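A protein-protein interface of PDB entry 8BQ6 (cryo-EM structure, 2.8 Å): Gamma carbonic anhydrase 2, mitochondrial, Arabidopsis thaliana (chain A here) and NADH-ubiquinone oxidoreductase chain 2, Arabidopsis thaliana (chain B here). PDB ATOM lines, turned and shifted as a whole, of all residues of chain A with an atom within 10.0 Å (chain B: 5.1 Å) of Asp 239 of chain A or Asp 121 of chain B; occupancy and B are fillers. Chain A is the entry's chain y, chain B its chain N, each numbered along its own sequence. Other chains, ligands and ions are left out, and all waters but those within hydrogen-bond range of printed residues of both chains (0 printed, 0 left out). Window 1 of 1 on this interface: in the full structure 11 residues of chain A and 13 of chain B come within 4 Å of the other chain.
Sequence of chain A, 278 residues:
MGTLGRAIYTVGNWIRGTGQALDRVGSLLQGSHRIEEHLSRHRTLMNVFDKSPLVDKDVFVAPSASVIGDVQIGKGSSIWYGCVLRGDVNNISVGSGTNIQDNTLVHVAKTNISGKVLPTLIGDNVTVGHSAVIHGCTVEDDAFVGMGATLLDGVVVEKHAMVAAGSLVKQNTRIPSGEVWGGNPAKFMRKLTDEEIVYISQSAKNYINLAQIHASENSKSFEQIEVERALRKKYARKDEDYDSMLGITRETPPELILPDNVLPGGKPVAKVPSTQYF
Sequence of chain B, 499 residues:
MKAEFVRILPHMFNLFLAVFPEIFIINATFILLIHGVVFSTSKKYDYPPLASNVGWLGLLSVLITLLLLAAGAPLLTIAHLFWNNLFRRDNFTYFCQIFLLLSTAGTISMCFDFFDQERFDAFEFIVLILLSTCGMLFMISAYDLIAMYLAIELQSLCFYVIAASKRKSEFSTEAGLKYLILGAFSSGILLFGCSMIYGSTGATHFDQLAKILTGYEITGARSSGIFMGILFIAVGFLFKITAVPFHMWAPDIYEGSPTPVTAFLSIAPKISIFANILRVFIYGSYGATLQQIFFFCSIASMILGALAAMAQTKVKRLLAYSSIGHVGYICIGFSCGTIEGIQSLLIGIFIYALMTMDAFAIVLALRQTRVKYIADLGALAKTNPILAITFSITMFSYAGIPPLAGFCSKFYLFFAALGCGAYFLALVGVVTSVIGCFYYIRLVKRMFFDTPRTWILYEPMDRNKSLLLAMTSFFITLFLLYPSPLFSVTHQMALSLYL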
ATOM      1  N   LYS A 234      -5.192  10.685  26.031  1.00  0.00           N
ATOM      2  CA  LYS A 234      -4.867  10.098  24.732  1.00  0.00           C
ATOM      3  C   LYS A 234      -6.111   9.634  23.986  1.00  0.00           C
ATOM      4  O   LYS A 234      -6.188   9.754  22.757  1.00  0.00           O
ATOM      5  CB  LYS A 234      -3.911   8.925  24.930  1.00  0.00           C
ATOM      6  CG  LYS A 234      -3.343   8.330  23.656  1.00  0.00           C
ATOM      7  CD  LYS A 234      -1.827   8.371  23.671  1.00  0.00           C
ATOM      8  CE  LYS A 234      -1.228   7.330  22.729  1.00  0.00           C
ATOM      9  NZ  LYS A 234      -1.588   7.561  21.303  1.00  0.00           N
ATOM     10  N   TYR A 235      -7.081   9.070  24.700  1.00  0.00           N
ATOM     11  CA  TYR A 235      -8.244   8.448  24.084  1.00  0.00           C
ATOM     12  C   TYR A 235      -9.511   9.268  24.244  1.00  0.00           C
ATOM     13  O   TYR A 235     -10.608   8.726  24.087  1.00  0.00           O
ATOM     14  CB  TYR A 235      -8.449   7.049  24.662  1.00  0.00           C
ATOM     15  CG  TYR A 235      -7.411   6.098  24.158  1.00  0.00           C
ATOM     16  CD1 TYR A 235      -7.609   5.386  22.989  1.00  0.00           C
ATOM     17  CD2 TYR A 235      -6.198   5.969  24.810  1.00  0.00           C
ATOM     18  CE1 TYR A 235      -6.648   4.542  22.510  1.00  0.00           C
ATOM     19  CE2 TYR A 235      -5.232   5.129  24.339  1.00  0.00           C
ATOM     20  CZ  TYR A 235      -5.459   4.418  23.189  1.00  0.00           C
ATOM     21  OH  TYR A 235      -4.486   3.575  22.718  1.00  0.00           O
ATOM     22  N   ALA A 236      -9.388  10.560  24.547  1.00  0.00           N
ATOM     23  CA  ALA A 236     -10.572  11.379  24.767  1.00  0.00           C
ATOM     24  C   ALA A 236     -11.317  11.665  23.470  1.00  0.00           C
ATOM     25  O   ALA A 236     -12.552  11.677  23.459  1.00  0.00           O
ATOM     26  CB  ALA A 236     -10.184  12.686  25.454  1.00  0.00           C
ATOM     27  N   ARG A 237     -10.596  11.909  22.381  1.00  0.00           N
ATOM     28  CA  ARG A 237     -11.193  12.130  21.072  1.00  0.00           C
ATOM     29  C   ARG A 237     -10.611  11.114  20.099  1.00  0.00           C
ATOM     30  O   ARG A 237      -9.827  10.241  20.479  1.00  0.00           O
ATOM     31  CB  ARG A 237     -10.954  13.562  20.581  1.00  0.00           C
ATOM     32  CG  ARG A 237     -11.587  14.630  21.444  1.00  0.00           C
ATOM     33  CD  ARG A 237     -13.102  14.548  21.397  1.00  0.00           C
ATOM     34  NE  ARG A 237     -13.723  15.589  22.206  1.00  0.00           N
ATOM     35  CZ  ARG A 237     -15.007  15.620  22.531  1.00  0.00           C
ATOM     36  NH1 ARG A 237     -15.836  14.655  22.169  1.00  0.00           N
ATOM     37  NH2 ARG A 237     -15.473  16.646  23.239  1.00  0.00           N
ATOM     38  N   LYS A 238     -10.992  11.217  18.829  1.00  0.00           N
ATOM     39  CA  LYS A 238     -10.483  10.263  17.859  1.00  0.00           C
ATOM     40  C   LYS A 238     -10.456  10.875  16.468  1.00  0.00           C
ATOM     41  O   LYS A 238     -11.129  11.869  16.185  1.00  0.00           O
ATOM     42  CB  LYS A 238     -11.315   8.978  17.839  1.00  0.00           C
ATOM     43  CG  LYS A 238     -12.761   9.175  17.440  1.00  0.00           C
ATOM     44  CD  LYS A 238     -13.490   7.845  17.454  1.00  0.00           C
ATOM     45  CE  LYS A 238     -14.946   7.991  17.061  1.00  0.00           C
ATOM     46  NZ  LYS A 238     -15.690   8.801  18.062  1.00  0.00           N
ATOM     47  N   ASP A 239      -9.642  10.263  15.604  1.00  0.00           N
ATOM     48  CA  ASP A 239      -9.656  10.496  14.159  1.00  0.00           C
ATOM     49  C   ASP A 239      -9.667   9.125  13.500  1.00  0.00           C
ATOM     50  O   ASP A 239      -8.617   8.582  13.152  1.00  0.00           O
ATOM     51  CB  ASP A 239      -8.471  11.317  13.713  1.00  0.00           C
ATOM     52  CG  ASP A 239      -8.623  11.844  12.299  1.00  0.00           C
ATOM     53  OD1 ASP A 239      -9.622  11.507  11.635  1.00  0.00           O
ATOM     54  OD2 ASP A 239      -7.755  12.624  11.859  1.00  0.00           O
ATOM     55  N   GLU A 240     -10.861   8.562  13.325  1.00  0.00           N
ATOM     56  CA  GLU A 240     -10.949   7.250  12.701  1.00  0.00           C
ATOM     57  C   GLU A 240     -10.714   7.324  11.201  1.00  0.00           C
ATOM     58  O   GLU A 240     -10.334   6.323  10.584  1.00  0.00           O
ATOM     59  CB  GLU A 240     -12.296   6.612  13.021  1.00  0.00           C
ATOM     60  CG  GLU A 240     -12.592   6.654  14.497  1.00  0.00           C
ATOM     61  CD  GLU A 240     -13.361   5.445  14.988  1.00  0.00           C
ATOM     62  OE1 GLU A 240     -12.745   4.607  15.679  1.00  0.00           O
ATOM     63  OE2 GLU A 240     -14.576   5.346  14.723  1.00  0.00           O
ATOM     64  N   ASP A 241     -10.901   8.497  10.603  1.00  0.00           N
ATOM     65  CA  ASP A 241     -10.579   8.654   9.192  1.00  0.00           C
ATOM     66  C   ASP A 241      -9.079   8.538   8.945  1.00  0.00           C
ATOM     67  O   ASP A 241      -8.638   7.770   8.077  1.00  0.00           O
ATOM     68  CB  ASP A 241     -11.094   9.997   8.702  1.00  0.00           C
ATOM     69  CG  ASP A 241     -11.205  10.050   7.217  1.00  0.00           C
ATOM     70  OD1 ASP A 241     -11.186   8.975   6.583  1.00  0.00           O
ATOM     71  OD2 ASP A 241     -11.308  11.164   6.684  1.00  0.00           O
ATOM     72  N   TYR A 242      -8.277   9.289   9.701  1.00  0.00           N
ATOM     73  CA  TYR A 242      -6.833   9.193   9.547  1.00  0.00           C
ATOM     74  C   TYR A 242      -6.322   7.823   9.958  1.00  0.00           C
ATOM     75  O   TYR A 242      -5.353   7.321   9.375  1.00  0.00           O
ATOM     76  CB  TYR A 242      -6.133  10.280  10.357  1.00  0.00           C
ATOM     77  CG  TYR A 242      -4.740  10.548   9.865  1.00  0.00           C
ATOM     78  CD1 TYR A 242      -4.529  11.219   8.676  1.00  0.00           C
ATOM     79  CD2 TYR A 242      -3.638  10.113  10.578  1.00  0.00           C
ATOM     80  CE1 TYR A 242      -3.266  11.456   8.214  1.00  0.00           C
ATOM     81  CE2 TYR A 242      -2.367  10.348  10.124  1.00  0.00           C
ATOM     82  CZ  TYR A 242      -2.186  11.022   8.939  1.00  0.00           C
ATOM     83  OH  TYR A 242      -0.919  11.268   8.468  1.00  0.00           O
ATOM     84  N   ASP A 243      -6.959   7.207  10.954  1.00  0.00           N
ATOM     85  CA  ASP A 243      -6.609   5.843  11.327  1.00  0.00           C
ATOM     86  C   ASP A 243      -6.857   4.870  10.184  1.00  0.00           C
ATOM     87  O   ASP A 243      -6.051   3.963   9.950  1.00  0.00           O
ATOM     88  CB  ASP A 243      -7.402   5.413  12.556  1.00  0.00           C
ATOM     89  CG  ASP A 243      -6.789   5.906  13.836  1.00  0.00           C
ATOM     90  OD1 ASP A 243      -7.542   6.331  14.732  1.00  0.00           O
ATOM     91  OD2 ASP A 243      -5.549   5.865  13.947  1.00  0.00           O
ATOM     92  N   SER A 244      -7.980   5.018   9.480  1.00  0.00           N
ATOM     93  CA  SER A 244      -8.238   4.126   8.356  1.00  0.00           C
ATOM     94  C   SER A 244      -7.255   4.386   7.226  1.00  0.00           C
ATOM     95  O   SER A 244      -6.887   3.463   6.490  1.00  0.00           O
ATOM     96  CB  SER A 244      -9.678   4.272   7.869  1.00  0.00           C
ATOM     97  OG  SER A 244      -9.773   5.225   6.829  1.00  0.00           O
ATOM     98  N   MET A 245      -6.813   5.638   7.072  1.00  0.00           N
ATOM     99  CA  MET A 245      -5.755   5.914   6.103  1.00  0.00           C
ATOM    100  C   MET A 245      -4.462   5.203   6.482  1.00  0.00           C
ATOM    101  O   MET A 245      -3.790   4.620   5.622  1.00  0.00           O
ATOM    102  CB  MET A 245      -5.510   7.415   5.973  1.00  0.00           C
ATOM    103  CG  MET A 245      -4.551   7.759   4.840  1.00  0.00           C
ATOM    104  SD  MET A 245      -3.614   9.269   5.106  1.00  0.00           S
ATOM    105  CE  MET A 245      -2.396   8.661   6.262  1.00  0.00           C
ATOM    106  N   LEU A 246      -4.089   5.249   7.763  1.00  0.00           N
ATOM    107  CA  LEU A 246      -2.929   4.511   8.248  1.00  0.00           C
ATOM    108  C   LEU A 246      -3.164   3.009   8.297  1.00  0.00           C
ATOM    109  O   LEU A 246      -2.194   2.251   8.396  1.00  0.00           O
ATOM    110  CB  LEU A 246      -2.540   4.994   9.643  1.00  0.00           C
ATOM    111  CG  LEU A 246      -1.859   6.355   9.747  1.00  0.00           C
ATOM    112  CD1 LEU A 246      -1.997   6.900  11.157  1.00  0.00           C
ATOM    113  CD2 LEU A 246      -0.404   6.235   9.359  1.00  0.00           C
ATOM    114  N   GLY A 247      -4.415   2.567   8.233  1.00  0.00           N
ATOM    115  CA  GLY A 247      -4.739   1.163   8.395  1.00  0.00           C
ATOM    116  C   GLY A 247      -4.495   0.620   9.786  1.00  0.00           C
ATOM    117  O   GLY A 247      -3.972  -0.490   9.930  1.00  0.00           O
ATOM    118  N   ILE A 248      -4.859   1.376  10.820  1.00  0.00           N
ATOM    119  CA  ILE A 248      -4.709   0.927  12.196  1.00  0.00           C
ATOM    120  C   ILE A 248      -6.037   1.117  12.910  1.00  0.00           C
ATOM    121  O   ILE A 248      -6.916   1.849  12.457  1.00  0.00           O
ATOM    122  CB  ILE A 248      -3.587   1.670  12.946  1.00  0.00           C
ATOM    123  CG1 ILE A 248      -3.968   3.131  13.141  1.00  0.00           C
ATOM    124  CG2 ILE A 248      -2.283   1.567  12.196  1.00  0.00           C
ATOM    125  CD1 ILE A 248      -3.121   3.829  14.135  1.00  0.00           C
ATOM    126  N   THR A 249      -6.182   0.425  14.035  1.00  0.00           N
ATOM    127  CA  THR A 249      -7.399   0.486  14.835  1.00  0.00           C
ATOM    128  C   THR A 249      -6.996   0.725  16.279  1.00  0.00           C
ATOM    129  O   THR A 249      -6.508  -0.189  16.949  1.00  0.00           O
ATOM    130  CB  THR A 249      -8.219  -0.795  14.704  1.00  0.00           C
ATOM    131  OG1 THR A 249      -8.323  -1.153  13.322  1.00  0.00           O
ATOM    132  CG2 THR A 249      -9.614  -0.601  15.285  1.00  0.00           C
ATOM    133  N   ARG A 250      -7.194   1.946  16.751  1.00  0.00           N
ATOM    134  CA  ARG A 250      -6.867   2.275  18.126  1.00  0.00           C
ATOM    135  C   ARG A 250      -7.916   1.677  19.049  1.00  0.00           C
ATOM    136  O   ARG A 250      -9.120   1.850  18.834  1.00  0.00           O
ATOM    137  CB  ARG A 250      -6.780   3.787  18.298  1.00  0.00           C
ATOM    138  CG  ARG A 250      -5.926   4.443  17.233  1.00  0.00           C
ATOM    139  CD  ARG A 250      -5.476   5.815  17.666  1.00  0.00           C
ATOM    140  NE  ARG A 250      -4.712   6.494  16.629  1.00  0.00           N
ATOM    141  CZ  ARG A 250      -3.388   6.491  16.550  1.00  0.00           C
ATOM    142  NH1 ARG A 250      -2.646   5.840  17.429  1.00  0.00           N
ATOM    143  NH2 ARG A 250      -2.795   7.165  15.569  1.00  0.00           N
ATOM    144  N   PRO B  49      -0.130  11.090  16.300  1.00  0.00           N
ATOM    145  CA  PRO B  49      -0.631  12.217  15.508  1.00  0.00           C
ATOM    146  C   PRO B  49       0.414  13.318  15.473  1.00  0.00           C
ATOM    147  O   PRO B  49       0.890  13.775  16.514  1.00  0.00           O
ATOM    148  CB  PRO B  49      -1.881  12.660  16.271  1.00  0.00           C
ATOM    149  CG  PRO B  49      -2.299  11.489  17.035  1.00  0.00           C
ATOM    150  CD  PRO B  49      -1.059  10.718  17.378  1.00  0.00           C
ATOM    151  N   LEU B  50       0.769  13.754  14.269  1.00  0.00           N
ATOM    152  CA  LEU B  50       1.840  14.729  14.112  1.00  0.00           C
ATOM    153  C   LEU B  50       1.361  16.074  13.589  1.00  0.00           C
ATOM    154  O   LEU B  50       2.194  16.908  13.219  1.00  0.00           O
ATOM    155  CB  LEU B  50       2.929  14.169  13.197  1.00  0.00           C
ATOM    156  CG  LEU B  50       3.669  13.009  13.856  1.00  0.00           C
ATOM    157  CD1 LEU B  50       4.669  12.374  12.916  1.00  0.00           C
ATOM    158  CD2 LEU B  50       4.345  13.500  15.116  1.00  0.00           C
ATOM    159  N   ALA B  51       0.052  16.320  13.561  1.00  0.00           N
ATOM    160  CA  ALA B  51      -0.435  17.561  12.971  1.00  0.00           C
ATOM    161  C   ALA B  51       0.041  18.779  13.756  1.00  0.00           C
ATOM    162  O   ALA B  51       0.483  19.769  13.165  1.00  0.00           O
ATOM    163  CB  ALA B  51      -1.958  17.536  12.870  1.00  0.00           C
ATOM    164  N   PHE B 115      -6.492  20.927  15.617  1.00  0.00           N
ATOM    165  CA  PHE B 115      -5.764  19.670  15.468  1.00  0.00           C
ATOM    166  C   PHE B 115      -5.974  18.762  16.673  1.00  0.00           C
ATOM    167  O   PHE B 115      -6.180  17.553  16.527  1.00  0.00           O
ATOM    168  CB  PHE B 115      -4.267  19.909  15.269  1.00  0.00           C
ATOM    169  CG  PHE B 115      -3.920  20.620  14.002  1.00  0.00           C
ATOM    170  CD1 PHE B 115      -4.619  20.375  12.839  1.00  0.00           C
ATOM    171  CD2 PHE B 115      -2.827  21.466  13.956  1.00  0.00           C
ATOM    172  CE1 PHE B 115      -4.282  21.011  11.674  1.00  0.00           C
ATOM    173  CE2 PHE B 115      -2.480  22.099  12.792  1.00  0.00           C
ATOM    174  CZ  PHE B 115      -3.208  21.871  11.646  1.00  0.00           C
ATOM    175  N   ARG B 119      -9.270  16.081  16.760  1.00  0.00           N
ATOM    176  CA  ARG B 119      -8.340  15.085  16.270  1.00  0.00           C
ATOM    177  C   ARG B 119      -8.416  15.037  14.747  1.00  0.00           C
ATOM    178  O   ARG B 119      -9.001  14.154  14.131  1.00  0.00           O
ATOM    179  CB  ARG B 119      -8.579  13.732  16.930  1.00  0.00           C
ATOM    180  CG  ARG B 119      -8.228  13.812  18.384  1.00  0.00           C
ATOM    181  CD  ARG B 119      -6.769  13.521  18.613  1.00  0.00           C
ATOM    182  NE  ARG B 119      -6.261  12.513  17.694  1.00  0.00           N
ATOM    183  CZ  ARG B 119      -6.343  11.212  17.921  1.00  0.00           C
ATOM    184  NH1 ARG B 119      -6.963  10.737  18.988  1.00  0.00           N
ATOM    185  NH2 ARG B 119      -5.790  10.366  17.058  1.00  0.00           N
ATOM    186  N   PHE B 120      -7.936  16.130  14.181  1.00  0.00           N
ATOM    187  CA  PHE B 120      -7.507  16.159  12.796  1.00  0.00           C
ATOM    188  C   PHE B 120      -6.011  15.883  12.848  1.00  0.00           C
ATOM    189  O   PHE B 120      -5.227  16.747  13.241  1.00  0.00           O
ATOM    190  CB  PHE B 120      -7.839  17.505  12.166  1.00  0.00           C
ATOM    191  CG  PHE B 120      -7.571  17.561  10.706  1.00  0.00           C
ATOM    192  CD1 PHE B 120      -6.308  17.843  10.228  1.00  0.00           C
ATOM    193  CD2 PHE B 120      -8.582  17.286   9.806  1.00  0.00           C
ATOM    194  CE1 PHE B 120      -6.066  17.874   8.878  1.00  0.00           C
ATOM    195  CE2 PHE B 120      -8.343  17.315   8.459  1.00  0.00           C
ATOM    196  CZ  PHE B 120      -7.084  17.611   7.993  1.00  0.00           C
ATOM    197  N   ASP B 121      -5.609  14.657  12.506  1.00  0.00           N
ATOM    198  CA  ASP B 121      -4.227  14.233  12.709  1.00  0.00           C
ATOM    199  C   ASP B 121      -3.346  14.358  11.475  1.00  0.00           C
ATOM    200  O   ASP B 121      -2.149  14.069  11.570  1.00  0.00           O
ATOM    201  CB  ASP B 121      -4.139  12.779  13.186  1.00  0.00           C
ATOM    202  CG  ASP B 121      -5.040  12.476  14.353  1.00  0.00           C
ATOM    203  OD1 ASP B 121      -5.152  13.314  15.265  1.00  0.00           O
ATOM    204  OD2 ASP B 121      -5.569  11.354  14.404  1.00  0.00           O
ATOM    205  N   ALA B 122      -3.887  14.758  10.332  1.00  0.00           N
ATOM    206  CA  ALA B 122      -3.112  14.735   9.097  1.00  0.00           C
ATOM    207  C   ALA B 122      -2.103  15.876   9.092  1.00  0.00           C
ATOM    208  O   ALA B 122      -2.480  17.050   9.057  1.00  0.00           O
ATOM    209  CB  ALA B 122      -4.037  14.821   7.888  1.00  0.00           C
ATOM    210  N   PHE B 123      -0.816  15.535   9.129  1.00  0.00           N
ATOM    211  CA  PHE B 123       0.215  16.554   9.008  1.00  0.00           C
ATOM    212  C   PHE B 123       0.336  17.085   7.586  1.00  0.00           C
ATOM    213  O   PHE B 123       0.882  18.175   7.393  1.00  0.00           O
ATOM    214  CB  PHE B 123       1.561  16.001   9.474  1.00  0.00           C
ATOM    215  CG  PHE B 123       2.187  15.055   8.498  1.00  0.00           C
ATOM    216  CD1 PHE B 123       1.939  13.700   8.578  1.00  0.00           C
ATOM    217  CD2 PHE B 123       3.008  15.520   7.489  1.00  0.00           C
ATOM    218  CE1 PHE B 123       2.504  12.828   7.676  1.00  0.00           C
ATOM    219  CE2 PHE B 123       3.566  14.653   6.587  1.00  0.00           C
ATOM    220  CZ  PHE B 123       3.313  13.303   6.681  1.00  0.00           C
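Lys 234 of chain A touches Arg 119 of chain B. Lys 238 of chain A touches Arg 119 of chain B (O to CB, 3.2 Å). Asp 239 of chain A touches Phe 120 of chain B (OD2 to CA, 3.7 Å). Asp 121 of chain B touches Tyr 242 of chain A (CB to CD2, 3.8 Å). Tyr 242 of chain A touches Ala 122 of chain B (CE1 to CA, 3.4 Å). Tyr 242 of chain A touches Phe 123 of chain B (OH to CD1, 3.8 Å).
Of the printed residues of chain B, Arg 237 of chain A touches Arg 119. Of the printed residues of chain B, Lys 238 of chain A touches Arg 119. Printed residues of chain B within 4 Å of Asp 239 of chain A: Arg 119 (2.9 Å), Phe 120 (3.7 Å) and Asp 121 (3.0 Å). Arg 119 of chain B touches just these residues of chain A: Lys 234, Arg 237, Lys 238 and Asp 239. Of chain A, only Asp 239 (3.7 Å) comes within 4 Å of Phe 120 of chain B. Asp 121 of chain B touches just these residues of chain A: Asp 239 and Tyr 242. Of chain A, only Tyr 242 comes within 4 Å of Ala 122 of chain B. The nearest residue of chain B that does not touch Asp 239 of chain A is Ala 122 of chain B (4.7 Å). The nearest residue of chain A that does not touch Asp 121 of chain B is Arg 250 of chain A (5.2 Å). The nearest printed residue of chain B that does not touch Tyr 242 of chain A is Pro 49 of chain B (6.0 Å).
The backbone NH (N) of Asp 241 of chain A sits close to the side-chain carboxylate (OD1) of Asp 239 of chain A. NE of Arg 119 of chain B lies within salt-bridge range of OD1 of Asp 121 of chain B, 2.8 Å away. The backbone carbonyl oxygen (O) of Phe 115 of chain B is in hydrogen-bond range of the backbone NH (N) of Phe 120 of chain B (3.3 Å). The backbone NH (N) of Tyr 242 of chain A sits at hydrogen-bond distance from the side-chain carboxylate (OD1) of Asp 239 of chain A.
Printed residues of chain A that touch a printed residue of chain B: Lys 234, Arg 237, Lys 238, Asp 239 and Tyr 242. Hydrophobic or aromatic side chains of chain B within 4 Å of the printed part of chain A: Ala 122 and Phe 123. Among the printed residues, no Asp or Glu carboxylate lies within 4 Å of a Lys or Arg side-chain nitrogen of the other chain.
The backbone carbonyl oxygen (O) of Arg 237 of chain A lies within hydrogen-bond range of the guanidinium group (NH1) of Arg 119 of chain B (3.3 Å). N of Asp 121 of chain B is in hydrogen-bond range of OD2 of Asp 239 of chain A, 3.0 Å away. The side-chain carboxylate of Asp 239 of chain A sits close to the backbone carbonyl oxygen of Arg 119 of chain B.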
